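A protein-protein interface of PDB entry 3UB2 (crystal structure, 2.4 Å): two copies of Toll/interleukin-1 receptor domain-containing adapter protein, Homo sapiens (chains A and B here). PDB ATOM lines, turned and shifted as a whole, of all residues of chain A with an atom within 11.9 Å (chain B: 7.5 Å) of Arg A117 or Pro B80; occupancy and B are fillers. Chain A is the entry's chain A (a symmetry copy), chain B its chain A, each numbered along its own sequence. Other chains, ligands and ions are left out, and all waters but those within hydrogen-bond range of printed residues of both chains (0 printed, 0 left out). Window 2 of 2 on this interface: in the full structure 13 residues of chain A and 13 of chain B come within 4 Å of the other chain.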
ATOM      1  N   ILE A  72      -0.887 -32.479 -24.101  1.00  0.00           N
ATOM      2  CA  ILE A  72      -0.245 -31.331 -24.713  1.00  0.00           C
ATOM      3  C   ILE A  72       0.729 -31.732 -25.828  1.00  0.00           C
ATOM      4  O   ILE A  72       1.836 -32.219 -25.582  1.00  0.00           O
ATOM      5  CB  ILE A  72       0.480 -30.498 -23.642  1.00  0.00           C
ATOM      6  CG1 ILE A  72      -0.514 -30.122 -22.535  1.00  0.00           C
ATOM      7  CG2 ILE A  72       1.101 -29.260 -24.266  1.00  0.00           C
ATOM      8  CD1 ILE A  72       0.081 -29.253 -21.449  1.00  0.00           C
ATOM      9  N   LEU A  77      -1.107 -27.199 -28.553  1.00  0.00           N
ATOM     10  CA  LEU A  77      -0.624 -25.850 -28.275  1.00  0.00           C
ATOM     11  C   LEU A  77      -1.001 -24.842 -29.360  1.00  0.00           C
ATOM     12  O   LEU A  77      -1.137 -23.648 -29.087  1.00  0.00           O
ATOM     13  CB  LEU A  77       0.894 -25.868 -28.081  1.00  0.00           C
ATOM     14  CG  LEU A  77       1.420 -26.615 -26.851  1.00  0.00           C
ATOM     15  CD1 LEU A  77       2.938 -26.698 -26.938  1.00  0.00           C
ATOM     16  CD2 LEU A  77       0.980 -25.904 -25.571  1.00  0.00           C
ATOM     17  N   MET A  86      -7.268 -25.884 -21.550  1.00  0.00           N
ATOM     18  CA  MET A  86      -6.164 -26.145 -20.638  1.00  0.00           C
ATOM     19  C   MET A  86      -6.244 -25.123 -19.516  1.00  0.00           C
ATOM     20  O   MET A  86      -6.046 -25.445 -18.349  1.00  0.00           O
ATOM     21  CB  MET A  86      -4.824 -25.988 -21.360  1.00  0.00           C
ATOM     22  CG  MET A  86      -3.614 -26.033 -20.440  1.00  0.00           C
ATOM     23  SD  MET A  86      -2.049 -25.874 -21.328  1.00  0.00           S
ATOM     24  CE  MET A  86      -1.339 -24.427 -20.528  1.00  0.00           C
ATOM     25  N   LEU A  90      -7.041 -25.844 -15.577  1.00  0.00           N
ATOM     26  CA  LEU A  90      -6.197 -25.396 -14.475  1.00  0.00           C
ATOM     27  C   LEU A  90      -6.875 -24.298 -13.655  1.00  0.00           C
ATOM     28  O   LEU A  90      -6.423 -23.967 -12.559  1.00  0.00           O
ATOM     29  CB  LEU A  90      -4.866 -24.878 -15.012  1.00  0.00           C
ATOM     30  CG  LEU A  90      -4.025 -25.905 -15.767  1.00  0.00           C
ATOM     31  CD1 LEU A  90      -2.854 -25.214 -16.441  1.00  0.00           C
ATOM     32  CD2 LEU A  90      -3.550 -26.976 -14.799  1.00  0.00           C
ATOM     33  N   PRO A  94      -5.533 -28.634 -10.028  1.00  0.00           N
ATOM     34  CA  PRO A  94      -4.184 -28.533  -9.496  1.00  0.00           C
ATOM     35  C   PRO A  94      -3.534 -27.190  -9.276  1.00  0.00           C
ATOM     36  O   PRO A  94      -2.908 -26.574 -10.135  1.00  0.00           O
ATOM     37  CB  PRO A  94      -3.408 -29.481 -10.391  1.00  0.00           C
ATOM     38  CG  PRO A  94      -4.333 -30.661 -10.354  1.00  0.00           C
ATOM     39  CD  PRO A  94      -5.721 -29.993 -10.578  1.00  0.00           C
ATOM     40  N   PRO A 102      -0.869 -32.723 -16.762  1.00  0.00           N
ATOM     41  CA  PRO A 102      -0.331 -32.341 -18.069  1.00  0.00           C
ATOM     42  C   PRO A 102       0.644 -33.411 -18.562  1.00  0.00           C
ATOM     43  O   PRO A 102       1.589 -33.770 -17.860  1.00  0.00           O
ATOM     44  CB  PRO A 102       0.385 -31.021 -17.779  1.00  0.00           C
ATOM     45  CG  PRO A 102      -0.295 -30.513 -16.534  1.00  0.00           C
ATOM     46  CD  PRO A 102      -0.453 -31.759 -15.730  1.00  0.00           C
ATOM     47  N   LEU A 104       3.192 -33.976 -21.548  1.00  0.00           N
ATOM     48  CA  LEU A 104       3.908 -33.403 -22.690  1.00  0.00           C
ATOM     49  C   LEU A 104       4.383 -34.497 -23.643  1.00  0.00           C
ATOM     50  O   LEU A 104       5.330 -35.219 -23.350  1.00  0.00           O
ATOM     51  CB  LEU A 104       5.102 -32.578 -22.203  1.00  0.00           C
ATOM     52  CG  LEU A 104       4.779 -31.201 -21.608  1.00  0.00           C
ATOM     53  CD1 LEU A 104       4.324 -30.275 -22.726  1.00  0.00           C
ATOM     54  CD2 LEU A 104       3.703 -31.314 -20.528  1.00  0.00           C
ATOM     55  N   SER A 108       9.432 -30.876 -28.240  1.00  0.00           N
ATOM     56  CA  SER A 108      10.783 -30.626 -27.790  1.00  0.00           C
ATOM     57  C   SER A 108      10.643 -29.857 -26.476  1.00  0.00           C
ATOM     58  O   SER A 108       9.811 -28.952 -26.369  1.00  0.00           O
ATOM     59  CB  SER A 108      11.510 -29.766 -28.817  1.00  0.00           C
ATOM     60  OG  SER A 108      12.605 -29.106 -28.216  1.00  0.00           O
ATOM     61  N   ARG A 109      11.440 -30.206 -25.474  1.00  0.00           N
ATOM     62  CA  ARG A 109      11.368 -29.519 -24.187  1.00  0.00           C
ATOM     63  C   ARG A 109      11.446 -27.998 -24.331  1.00  0.00           C
ATOM     64  O   ARG A 109      10.789 -27.261 -23.592  1.00  0.00           O
ATOM     65  CB  ARG A 109      12.492 -29.994 -23.268  1.00  0.00           C
ATOM     66  CG  ARG A 109      12.204 -31.270 -22.491  1.00  0.00           C
ATOM     67  CD  ARG A 109      13.496 -31.759 -21.869  1.00  0.00           C
ATOM     68  NE  ARG A 109      13.364 -32.096 -20.463  1.00  0.00           N
ATOM     69  CZ  ARG A 109      14.390 -32.266 -19.635  1.00  0.00           C
ATOM     70  NH1 ARG A 109      15.641 -32.131 -20.067  1.00  0.00           N
ATOM     71  NH2 ARG A 109      14.158 -32.559 -18.365  1.00  0.00           N
ATOM     72  N   ALA A 110      12.247 -27.532 -25.284  1.00  0.00           N
ATOM     73  CA  ALA A 110      12.407 -26.099 -25.511  1.00  0.00           C
ATOM     74  C   ALA A 110      11.093 -25.406 -25.928  1.00  0.00           C
ATOM     75  O   ALA A 110      10.968 -24.186 -25.823  1.00  0.00           O
ATOM     76  CB  ALA A 110      13.510 -25.853 -26.574  1.00  0.00           C
ATOM     77  N   ALA A 111      10.119 -26.189 -26.385  1.00  0.00           N
ATOM     78  CA  ALA A 111       8.829 -25.647 -26.816  1.00  0.00           C
ATOM     79  C   ALA A 111       7.750 -25.811 -25.745  1.00  0.00           C
ATOM     80  O   ALA A 111       6.575 -25.551 -25.994  1.00  0.00           O
ATOM     81  CB  ALA A 111       8.380 -26.329 -28.121  1.00  0.00           C
ATOM     82  N   TYR A 112       8.148 -26.249 -24.556  1.00  0.00           N
ATOM     83  CA  TYR A 112       7.191 -26.432 -23.469  1.00  0.00           C
ATOM     84  C   TYR A 112       6.696 -25.091 -22.924  1.00  0.00           C
ATOM     85  O   TYR A 112       7.447 -24.111 -22.877  1.00  0.00           O
ATOM     86  CB  TYR A 112       7.822 -27.215 -22.303  1.00  0.00           C
ATOM     87  CG  TYR A 112       8.054 -28.699 -22.533  1.00  0.00           C
ATOM     88  CD1 TYR A 112       7.815 -29.285 -23.777  1.00  0.00           C
ATOM     89  CD2 TYR A 112       8.509 -29.519 -21.496  1.00  0.00           C
ATOM     90  CE1 TYR A 112       8.023 -30.648 -23.979  1.00  0.00           C
ATOM     91  CE2 TYR A 112       8.719 -30.878 -21.690  1.00  0.00           C
ATOM     92  CZ  TYR A 112       8.470 -31.435 -22.928  1.00  0.00           C
ATOM     93  OH  TYR A 112       8.655 -32.786 -23.088  1.00  0.00           O
ATOM     94  N   PRO A 113       5.415 -25.028 -22.520  1.00  0.00           N
ATOM     95  CA  PRO A 113       4.842 -23.798 -21.960  1.00  0.00           C
ATOM     96  C   PRO A 113       5.644 -23.430 -20.700  1.00  0.00           C
ATOM     97  O   PRO A 113       5.659 -24.179 -19.729  1.00  0.00           O
ATOM     98  CB  PRO A 113       3.415 -24.211 -21.615  1.00  0.00           C
ATOM     99  CG  PRO A 113       3.091 -25.201 -22.686  1.00  0.00           C
ATOM    100  CD  PRO A 113       4.361 -26.030 -22.771  1.00  0.00           C
ATOM    101  N   PRO A 114       6.312 -22.268 -20.704  1.00  0.00           N
ATOM    102  CA  PRO A 114       7.123 -21.786 -19.577  1.00  0.00           C
ATOM    103  C   PRO A 114       6.558 -22.018 -18.172  1.00  0.00           C
ATOM    104  O   PRO A 114       7.300 -22.343 -17.240  1.00  0.00           O
ATOM    105  CB  PRO A 114       7.289 -20.305 -19.896  1.00  0.00           C
ATOM    106  CG  PRO A 114       7.394 -20.317 -21.409  1.00  0.00           C
ATOM    107  CD  PRO A 114       6.268 -21.268 -21.789  1.00  0.00           C
ATOM    108  N   GLU A 115       5.250 -21.858 -18.018  1.00  0.00           N
ATOM    109  CA  GLU A 115       4.624 -22.023 -16.710  1.00  0.00           C
ATOM    110  C   GLU A 115       4.813 -23.405 -16.098  1.00  0.00           C
ATOM    111  O   GLU A 115       4.814 -23.546 -14.876  1.00  0.00           O
ATOM    112  CB  GLU A 115       3.125 -21.696 -16.784  1.00  0.00           C
ATOM    113  CG  GLU A 115       2.339 -22.525 -17.796  1.00  0.00           C
ATOM    114  CD  GLU A 115       2.212 -21.855 -19.159  1.00  0.00           C
ATOM    115  OE1 GLU A 115       3.157 -21.157 -19.584  1.00  0.00           O
ATOM    116  OE2 GLU A 115       1.163 -22.039 -19.815  1.00  0.00           O
ATOM    117  N   LEU A 116       4.980 -24.419 -16.940  1.00  0.00           N
ATOM    118  CA  LEU A 116       5.149 -25.784 -16.451  1.00  0.00           C
ATOM    119  C   LEU A 116       6.349 -25.959 -15.536  1.00  0.00           C
ATOM    120  O   LEU A 116       6.378 -26.879 -14.723  1.00  0.00           O
ATOM    121  CB  LEU A 116       5.249 -26.767 -17.619  1.00  0.00           C
ATOM    122  CG  LEU A 116       3.958 -26.969 -18.411  1.00  0.00           C
ATOM    123  CD1 LEU A 116       4.188 -27.991 -19.503  1.00  0.00           C
ATOM    124  CD2 LEU A 116       2.843 -27.432 -17.482  1.00  0.00           C
ATOM    125  N   ARG A 117       7.336 -25.080 -15.668  1.00  0.00           N
ATOM    126  CA  ARG A 117       8.521 -25.157 -14.834  1.00  0.00           C
ATOM    127  C   ARG A 117       8.153 -25.114 -13.350  1.00  0.00           C
ATOM    128  O   ARG A 117       8.875 -25.653 -12.511  1.00  0.00           O
ATOM    129  CB  ARG A 117       9.481 -24.011 -15.161  1.00  0.00           C
ATOM    130  CG  ARG A 117      10.678 -23.942 -14.223  1.00  0.00           C
ATOM    131  CD  ARG A 117      11.629 -22.809 -14.582  1.00  0.00           C
ATOM    132  NE  ARG A 117      12.441 -22.397 -13.437  1.00  0.00           N
ATOM    133  CZ  ARG A 117      13.326 -21.403 -13.463  1.00  0.00           C
ATOM    134  NH1 ARG A 117      13.526 -20.716 -14.580  1.00  0.00           N
ATOM    135  NH2 ARG A 117      14.000 -21.084 -12.364  1.00  0.00           N
ATOM    136  N   PHE A 118       7.027 -24.476 -13.034  1.00  0.00           N
ATOM    137  CA  PHE A 118       6.558 -24.365 -11.652  1.00  0.00           C
ATOM    138  C   PHE A 118       5.342 -25.241 -11.401  1.00  0.00           C
ATOM    139  O   PHE A 118       4.624 -25.051 -10.420  1.00  0.00           O
ATOM    140  CB  PHE A 118       6.192 -22.916 -11.309  1.00  0.00           C
ATOM    141  CG  PHE A 118       7.341 -21.957 -11.406  1.00  0.00           C
ATOM    142  CD1 PHE A 118       7.583 -21.261 -12.585  1.00  0.00           C
ATOM    143  CD2 PHE A 118       8.205 -21.772 -10.322  1.00  0.00           C
ATOM    144  CE1 PHE A 118       8.669 -20.389 -12.692  1.00  0.00           C
ATOM    145  CE2 PHE A 118       9.299 -20.903 -10.413  1.00  0.00           C
ATOM    146  CZ  PHE A 118       9.533 -20.208 -11.601  1.00  0.00           C
ATOM    147  N   MET A 119       5.118 -26.206 -12.284  1.00  0.00           N
ATOM    148  CA  MET A 119       3.974 -27.091 -12.155  1.00  0.00           C
ATOM    149  C   MET A 119       4.345 -28.555 -12.330  1.00  0.00           C
ATOM    150  O   MET A 119       5.411 -28.891 -12.851  1.00  0.00           O
ATOM    151  CB  MET A 119       2.921 -26.728 -13.203  1.00  0.00           C
ATOM    152  CG  MET A 119       2.507 -25.264 -13.209  1.00  0.00           C
ATOM    153  SD  MET A 119       1.593 -24.853 -14.706  1.00  0.00           S
ATOM    154  CE  MET A 119       0.121 -25.865 -14.442  1.00  0.00           C
ATOM    155  N   TYR A 120       3.443 -29.425 -11.893  1.00  0.00           N
ATOM    156  CA  TYR A 120       3.644 -30.857 -12.031  1.00  0.00           C
ATOM    157  C   TYR A 120       3.210 -31.257 -13.438  1.00  0.00           C
ATOM    158  O   TYR A 120       2.225 -30.738 -13.960  1.00  0.00           O
ATOM    159  CB  TYR A 120       2.794 -31.620 -11.008  1.00  0.00           C
ATOM    160  CG  TYR A 120       2.773 -33.116 -11.248  1.00  0.00           C
ATOM    161  CD1 TYR A 120       3.894 -33.903 -10.979  1.00  0.00           C
ATOM    162  CD2 TYR A 120       1.647 -33.740 -11.787  1.00  0.00           C
ATOM    163  CE1 TYR A 120       3.896 -35.277 -11.243  1.00  0.00           C
ATOM    164  CE2 TYR A 120       1.638 -35.112 -12.057  1.00  0.00           C
ATOM    165  CZ  TYR A 120       2.768 -35.874 -11.781  1.00  0.00           C
ATOM    166  OH  TYR A 120       2.784 -37.230 -12.031  1.00  0.00           O
ATOM    167  N   TYR A 121       3.946 -32.173 -14.055  1.00  0.00           N
ATOM    168  CA  TYR A 121       3.599 -32.639 -15.392  1.00  0.00           C
ATOM    169  C   TYR A 121       4.379 -33.901 -15.705  1.00  0.00           C
ATOM    170  O   TYR A 121       5.405 -34.166 -15.090  1.00  0.00           O
ATOM    171  CB  TYR A 121       3.911 -31.576 -16.455  1.00  0.00           C
ATOM    172  CG  TYR A 121       5.386 -31.356 -16.713  1.00  0.00           C
ATOM    173  CD1 TYR A 121       6.135 -30.489 -15.914  1.00  0.00           C
ATOM    174  CD2 TYR A 121       6.038 -32.031 -17.746  1.00  0.00           C
ATOM    175  CE1 TYR A 121       7.498 -30.301 -16.136  1.00  0.00           C
ATOM    176  CE2 TYR A 121       7.402 -31.853 -17.977  1.00  0.00           C
ATOM    177  CZ  TYR A 121       8.125 -30.984 -17.171  1.00  0.00           C
ATOM    178  OH  TYR A 121       9.468 -30.792 -17.399  1.00  0.00           O
ATOM    179  N   VAL A 122       3.890 -34.672 -16.668  1.00  0.00           N
ATOM    180  CA  VAL A 122       4.547 -35.905 -17.056  1.00  0.00           C
ATOM    181  C   VAL A 122       5.165 -35.739 -18.435  1.00  0.00           C
ATOM    182  O   VAL A 122       4.502 -35.306 -19.384  1.00  0.00           O
ATOM    183  CB  VAL A 122       3.547 -37.071 -17.089  1.00  0.00           C
ATOM    184  CG1 VAL A 122       4.232 -38.342 -17.559  1.00  0.00           C
ATOM    185  CG2 VAL A 122       2.930 -37.252 -15.710  1.00  0.00           C
ATOM    186  N   ASP A 123       6.442 -36.078 -18.538  1.00  0.00           N
ATOM    187  CA  ASP A 123       7.144 -35.970 -19.799  1.00  0.00           C
ATOM    188  C   ASP A 123       6.910 -37.236 -20.621  1.00  0.00           C
ATOM    189  O   ASP A 123       6.966 -38.345 -20.090  1.00  0.00           O
ATOM    190  CB  ASP A 123       8.636 -35.767 -19.540  1.00  0.00           C
ATOM    191  CG  ASP A 123       9.346 -35.147 -20.720  1.00  0.00           C
ATOM    192  OD1 ASP A 123       9.508 -35.830 -21.750  1.00  0.00           O
ATOM    193  OD2 ASP A 123       9.733 -33.964 -20.613  1.00  0.00           O
ATOM    194  N   GLY B  75       9.096 -10.291 -23.152  1.00  0.00           N
ATOM    195  CA  GLY B  75       9.802 -10.698 -21.952  1.00  0.00           C
ATOM    196  C   GLY B  75       8.899 -11.443 -20.992  1.00  0.00           C
ATOM    197  O   GLY B  75       9.327 -12.374 -20.307  1.00  0.00           O
ATOM    198  N   PHE B  76       7.635 -11.037 -20.950  1.00  0.00           N
ATOM    199  CA  PHE B  76       6.658 -11.661 -20.071  1.00  0.00           C
ATOM    200  C   PHE B  76       6.393 -13.101 -20.483  1.00  0.00           C
ATOM    201  O   PHE B  76       6.429 -14.007 -19.652  1.00  0.00           O
ATOM    202  CB  PHE B  76       5.356 -10.854 -20.090  1.00  0.00           C
ATOM    203  CG  PHE B  76       4.303 -11.366 -19.149  1.00  0.00           C
ATOM    204  CD1 PHE B  76       3.442 -12.384 -19.530  1.00  0.00           C
ATOM    205  CD2 PHE B  76       4.166 -10.815 -17.883  1.00  0.00           C
ATOM    206  CE1 PHE B  76       2.454 -12.840 -18.665  1.00  0.00           C
ATOM    207  CE2 PHE B  76       3.183 -11.263 -17.015  1.00  0.00           C
ATOM    208  CZ  PHE B  76       2.327 -12.277 -17.403  1.00  0.00           C
ATOM    209  N   LEU B  77       6.129 -13.310 -21.769  1.00  0.00           N
ATOM    210  CA  LEU B  77       5.841 -14.646 -22.281  1.00  0.00           C
ATOM    211  C   LEU B  77       7.029 -15.601 -22.172  1.00  0.00           C
ATOM    212  O   LEU B  77       6.851 -16.816 -22.068  1.00  0.00           O
ATOM    213  CB  LEU B  77       5.370 -14.559 -23.735  1.00  0.00           C
ATOM    214  CG  LEU B  77       4.026 -13.866 -23.981  1.00  0.00           C
ATOM    215  CD1 LEU B  77       3.828 -13.695 -25.481  1.00  0.00           C
ATOM    216  CD2 LEU B  77       2.889 -14.682 -23.365  1.00  0.00           C
ATOM    217  N   GLN B  78       8.238 -15.050 -22.187  1.00  0.00           N
ATOM    218  CA  GLN B  78       9.439 -15.870 -22.085  1.00  0.00           C
ATOM    219  C   GLN B  78       9.741 -16.270 -20.645  1.00  0.00           C
ATOM    220  O   GLN B  78      10.418 -17.268 -20.406  1.00  0.00           O
ATOM    221  CB  GLN B  78      10.653 -15.125 -22.647  1.00  0.00           C
ATOM    222  CG  GLN B  78      10.620 -14.888 -24.148  1.00  0.00           C
ATOM    223  CD  GLN B  78      11.920 -14.290 -24.672  1.00  0.00           C
ATOM    224  OE1 GLN B  78      12.979 -14.919 -24.602  1.00  0.00           O
ATOM    225  NE2 GLN B  78      11.846 -13.069 -25.195  1.00  0.00           N
ATOM    226  N   ASP B  79       9.234 -15.493 -19.693  1.00  0.00           N
ATOM    227  CA  ASP B  79       9.480 -15.748 -18.280  1.00  0.00           C
ATOM    228  C   ASP B  79       8.519 -16.763 -17.657  1.00  0.00           C
ATOM    229  O   ASP B  79       7.312 -16.544 -17.583  1.00  0.00           O
ATOM    230  CB  ASP B  79       9.414 -14.428 -17.518  1.00  0.00           C
ATOM    231  CG  ASP B  79       9.965 -14.536 -16.117  1.00  0.00           C
ATOM    232  OD1 ASP B  79       9.535 -15.437 -15.365  1.00  0.00           O
ATOM    233  OD2 ASP B  79      10.828 -13.704 -15.770  1.00  0.00           O
ATOM    234  N   PRO B  80       9.061 -17.896 -17.187  1.00  0.00           N
ATOM    235  CA  PRO B  80       8.286 -18.973 -16.562  1.00  0.00           C
ATOM    236  C   PRO B  80       7.447 -18.514 -15.374  1.00  0.00           C
ATOM    237  O   PRO B  80       6.308 -18.951 -15.205  1.00  0.00           O
ATOM    238  CB  PRO B  80       9.360 -19.971 -16.146  1.00  0.00           C
ATOM    239  CG  PRO B  80      10.427 -19.761 -17.160  1.00  0.00           C
ATOM    240  CD  PRO B  80      10.485 -18.264 -17.284  1.00  0.00           C
ATOM    241  N   TRP B  81       8.020 -17.650 -14.542  1.00  0.00           N
ATOM    242  CA  TRP B  81       7.314 -17.140 -13.373  1.00  0.00           C
ATOM    243  C   TRP B  81       6.185 -16.189 -13.807  1.00  0.00           C
ATOM    244  O   TRP B  81       5.109 -16.176 -13.205  1.00  0.00           O
ATOM    245  CB  TRP B  81       8.305 -16.432 -12.438  1.00  0.00           C
ATOM    246  CG  TRP B  81       7.690 -15.914 -11.173  1.00  0.00           C
ATOM    247  CD1 TRP B  81       7.672 -14.617 -10.744  1.00  0.00           C
ATOM    248  CD2 TRP B  81       6.981 -16.672 -10.182  1.00  0.00           C
ATOM    249  NE1 TRP B  81       6.996 -14.520  -9.551  1.00  0.00           N
ATOM    250  CE2 TRP B  81       6.562 -15.767  -9.180  1.00  0.00           C
ATOM    251  CE3 TRP B  81       6.661 -18.031 -10.040  1.00  0.00           C
ATOM    252  CZ2 TRP B  81       5.834 -16.173  -8.052  1.00  0.00           C
ATOM    253  CZ3 TRP B  81       5.935 -18.437  -8.915  1.00  0.00           C
ATOM    254  CH2 TRP B  81       5.533 -17.509  -7.938  1.00  0.00           C
ATOM    255  N   CYS B  82       6.433 -15.402 -14.852  1.00  0.00           N
ATOM    256  CA  CYS B  82       5.412 -14.495 -15.372  1.00  0.00           C
ATOM    257  C   CYS B  82       4.230 -15.324 -15.864  1.00  0.00           C
ATOM    258  O   CYS B  82       3.083 -15.035 -15.528  1.00  0.00           O
ATOM    259  CB  CYS B  82       5.953 -13.669 -16.540  1.00  0.00           C
ATOM    260  SG  CYS B  82       7.216 -12.469 -16.092  1.00  0.00           S
ATOM    261  N   LYS B  83       4.522 -16.352 -16.661  1.00  0.00           N
ATOM    262  CA  LYS B  83       3.486 -17.227 -17.204  1.00  0.00           C
ATOM    263  C   LYS B  83       2.700 -17.919 -16.105  1.00  0.00           C
ATOM    264  O   LYS B  83       1.478 -18.041 -16.188  1.00  0.00           O
ATOM    265  CB  LYS B  83       4.101 -18.274 -18.138  1.00  0.00           C
ATOM    266  CG  LYS B  83       4.639 -17.689 -19.434  1.00  0.00           C
ATOM    267  CD  LYS B  83       3.576 -16.869 -20.171  1.00  0.00           C
ATOM    268  CE  LYS B  83       2.303 -17.667 -20.428  1.00  0.00           C
ATOM    269  NZ  LYS B  83       2.531 -18.820 -21.342  1.00  0.00           N
ATOM    270  N   TYR B  84       3.402 -18.377 -15.076  1.00  0.00           N
ATOM    271  CA  TYR B  84       2.744 -19.031 -13.956  1.00  0.00           C
ATOM    272  C   TYR B  84       1.837 -18.024 -13.231  1.00  0.00           C
ATOM    273  O   TYR B  84       0.723 -18.362 -12.834  1.00  0.00           O
ATOM    274  CB  TYR B  84       3.785 -19.586 -12.987  1.00  0.00           C
ATOM    275  CG  TYR B  84       3.179 -20.348 -11.838  1.00  0.00           C
ATOM    276  CD1 TYR B  84       2.561 -21.580 -12.046  1.00  0.00           C
ATOM    277  CD2 TYR B  84       3.217 -19.838 -10.539  1.00  0.00           C
ATOM    278  CE1 TYR B  84       1.994 -22.293 -10.988  1.00  0.00           C
ATOM    279  CE2 TYR B  84       2.651 -20.542  -9.468  1.00  0.00           C
ATOM    280  CZ  TYR B  84       2.041 -21.769  -9.703  1.00  0.00           C
ATOM    281  OH  TYR B  84       1.462 -22.463  -8.659  1.00  0.00           O
ATOM    282  N   GLN B  85       2.324 -16.794 -13.057  1.00  0.00           N
ATOM    283  CA  GLN B  85       1.547 -15.737 -12.404  1.00  0.00           C
ATOM    284  C   GLN B  85       0.301 -15.411 -13.227  1.00  0.00           C
ATOM    285  O   GLN B  85      -0.773 -15.165 -12.677  1.00  0.00           O
ATOM    286  CB  GLN B  85       2.401 -14.473 -12.226  1.00  0.00           C
ATOM    287  CG  GLN B  85       3.405 -14.574 -11.087  1.00  0.00           C
ATOM    288  CD  GLN B  85       2.737 -14.806  -9.739  1.00  0.00           C
ATOM    289  OE1 GLN B  85       1.971 -13.967  -9.261  1.00  0.00           O
ATOM    290  NE2 GLN B  85       3.023 -15.949  -9.123  1.00  0.00           N
ATOM    291  N   MET B  86       0.458 -15.409 -14.547  1.00  0.00           N
ATOM    292  CA  MET B  86      -0.654 -15.147 -15.450  1.00  0.00           C
ATOM    293  C   MET B  86      -1.685 -16.244 -15.235  1.00  0.00           C
ATOM    294  O   MET B  86      -2.884 -15.988 -15.198  1.00  0.00           O
ATOM    295  CB  MET B  86      -0.183 -15.185 -16.905  1.00  0.00           C
ATOM    296  CG  MET B  86      -1.310 -15.134 -17.924  1.00  0.00           C
ATOM    297  SD  MET B  86      -0.718 -15.150 -19.630  1.00  0.00           S
ATOM    298  CE  MET B  86      -1.555 -16.606 -20.277  1.00  0.00           C
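The side-chain carboxylate (OE1) of Glu A115 lies within salt-bridge range of the side-chain amino group (NZ) of Lys B83 (3.0 Å).
The side-chain carboxylate (OD1) of Asp B79 is in hydrogen-bond range of the backbone NH (N) of Trp B81 (2.8 Å).
O of Leu B77 touches CG of Pro A114, 3.6 Å away.
Pro A114 touches Pro B80 (O to CB, 3.3 Å).
CB of Pro A114 touches CG of Lys B83, 3.8 Å away.
Glu A115 touches Pro B80.
Tyr B84 touches Glu A115 (N to CB, 3.7 Å).
CD of Arg A117 touches CB of Pro B80, at 3.96 Å.
Phe A118 touches Pro B80.
Phe A118 touches Trp B81.
Phe A118 touches Tyr B84.
Met A119 touches Tyr B84 (CG to CE1, 3.7 Å).
Printed residues of chain B within 4 Å of Pro A114: Leu B77 (3.6 Å), Pro B80 (3.3 Å) and Lys B83 (3.8 Å).
Printed residues of chain B within 4 Å of Glu A115: Pro B80, Lys B83 and Tyr B84.
Of the printed residues of chain B, Phe A118 touches Pro B80, Trp B81 and Tyr B84.
No residue of chain A comes within 4 Å of Asp B79.
Pro B80 touches just these residues of chain A: Pro A114 (3.3 Å), Glu A115 (3.8 Å), Arg A117 (3.96 Å) and Phe A118 (3.5 Å).
Trp B81 touches just one residue of chain A: Phe A118 (3.4 Å).
Cys B82 touches none of the printed residues of chain A.
Of chain A, only Pro A114 (3.8 Å) and Glu A115 (3.0 Å) come within 4 Å of Lys B83.
The nearest residue of chain A that does not touch Pro B80 is Leu A116 (5.9 Å).
The nearest printed residue of chain A that does not touch Tyr B84 is Pro A114 (5.7 Å).
Of the 23 printed residues of chain A, 5 touch a printed residue of chain B.
Hydrophobic or aromatic side chains of chain A that line the printed part of chain B: Pro A114, Phe A118 and Met A119.
Printed residues of chain B that touch a printed residue of chain A: Leu B77, Pro B80, Trp B81, Lys B83 and Tyr B84.
Hydrophobic or aromatic side chains of chain B that line the printed part of chain A: Pro B80, Trp B81 and Tyr B84.
Among the printed residues, 11 pairs touch across the chains.
Among the printed residues, Asp or Glu carboxylates within 4 Å of a Lys or Arg side-chain nitrogen of the other chain: Glu A115 with Lys B83.
2 positions are printed for both chains.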
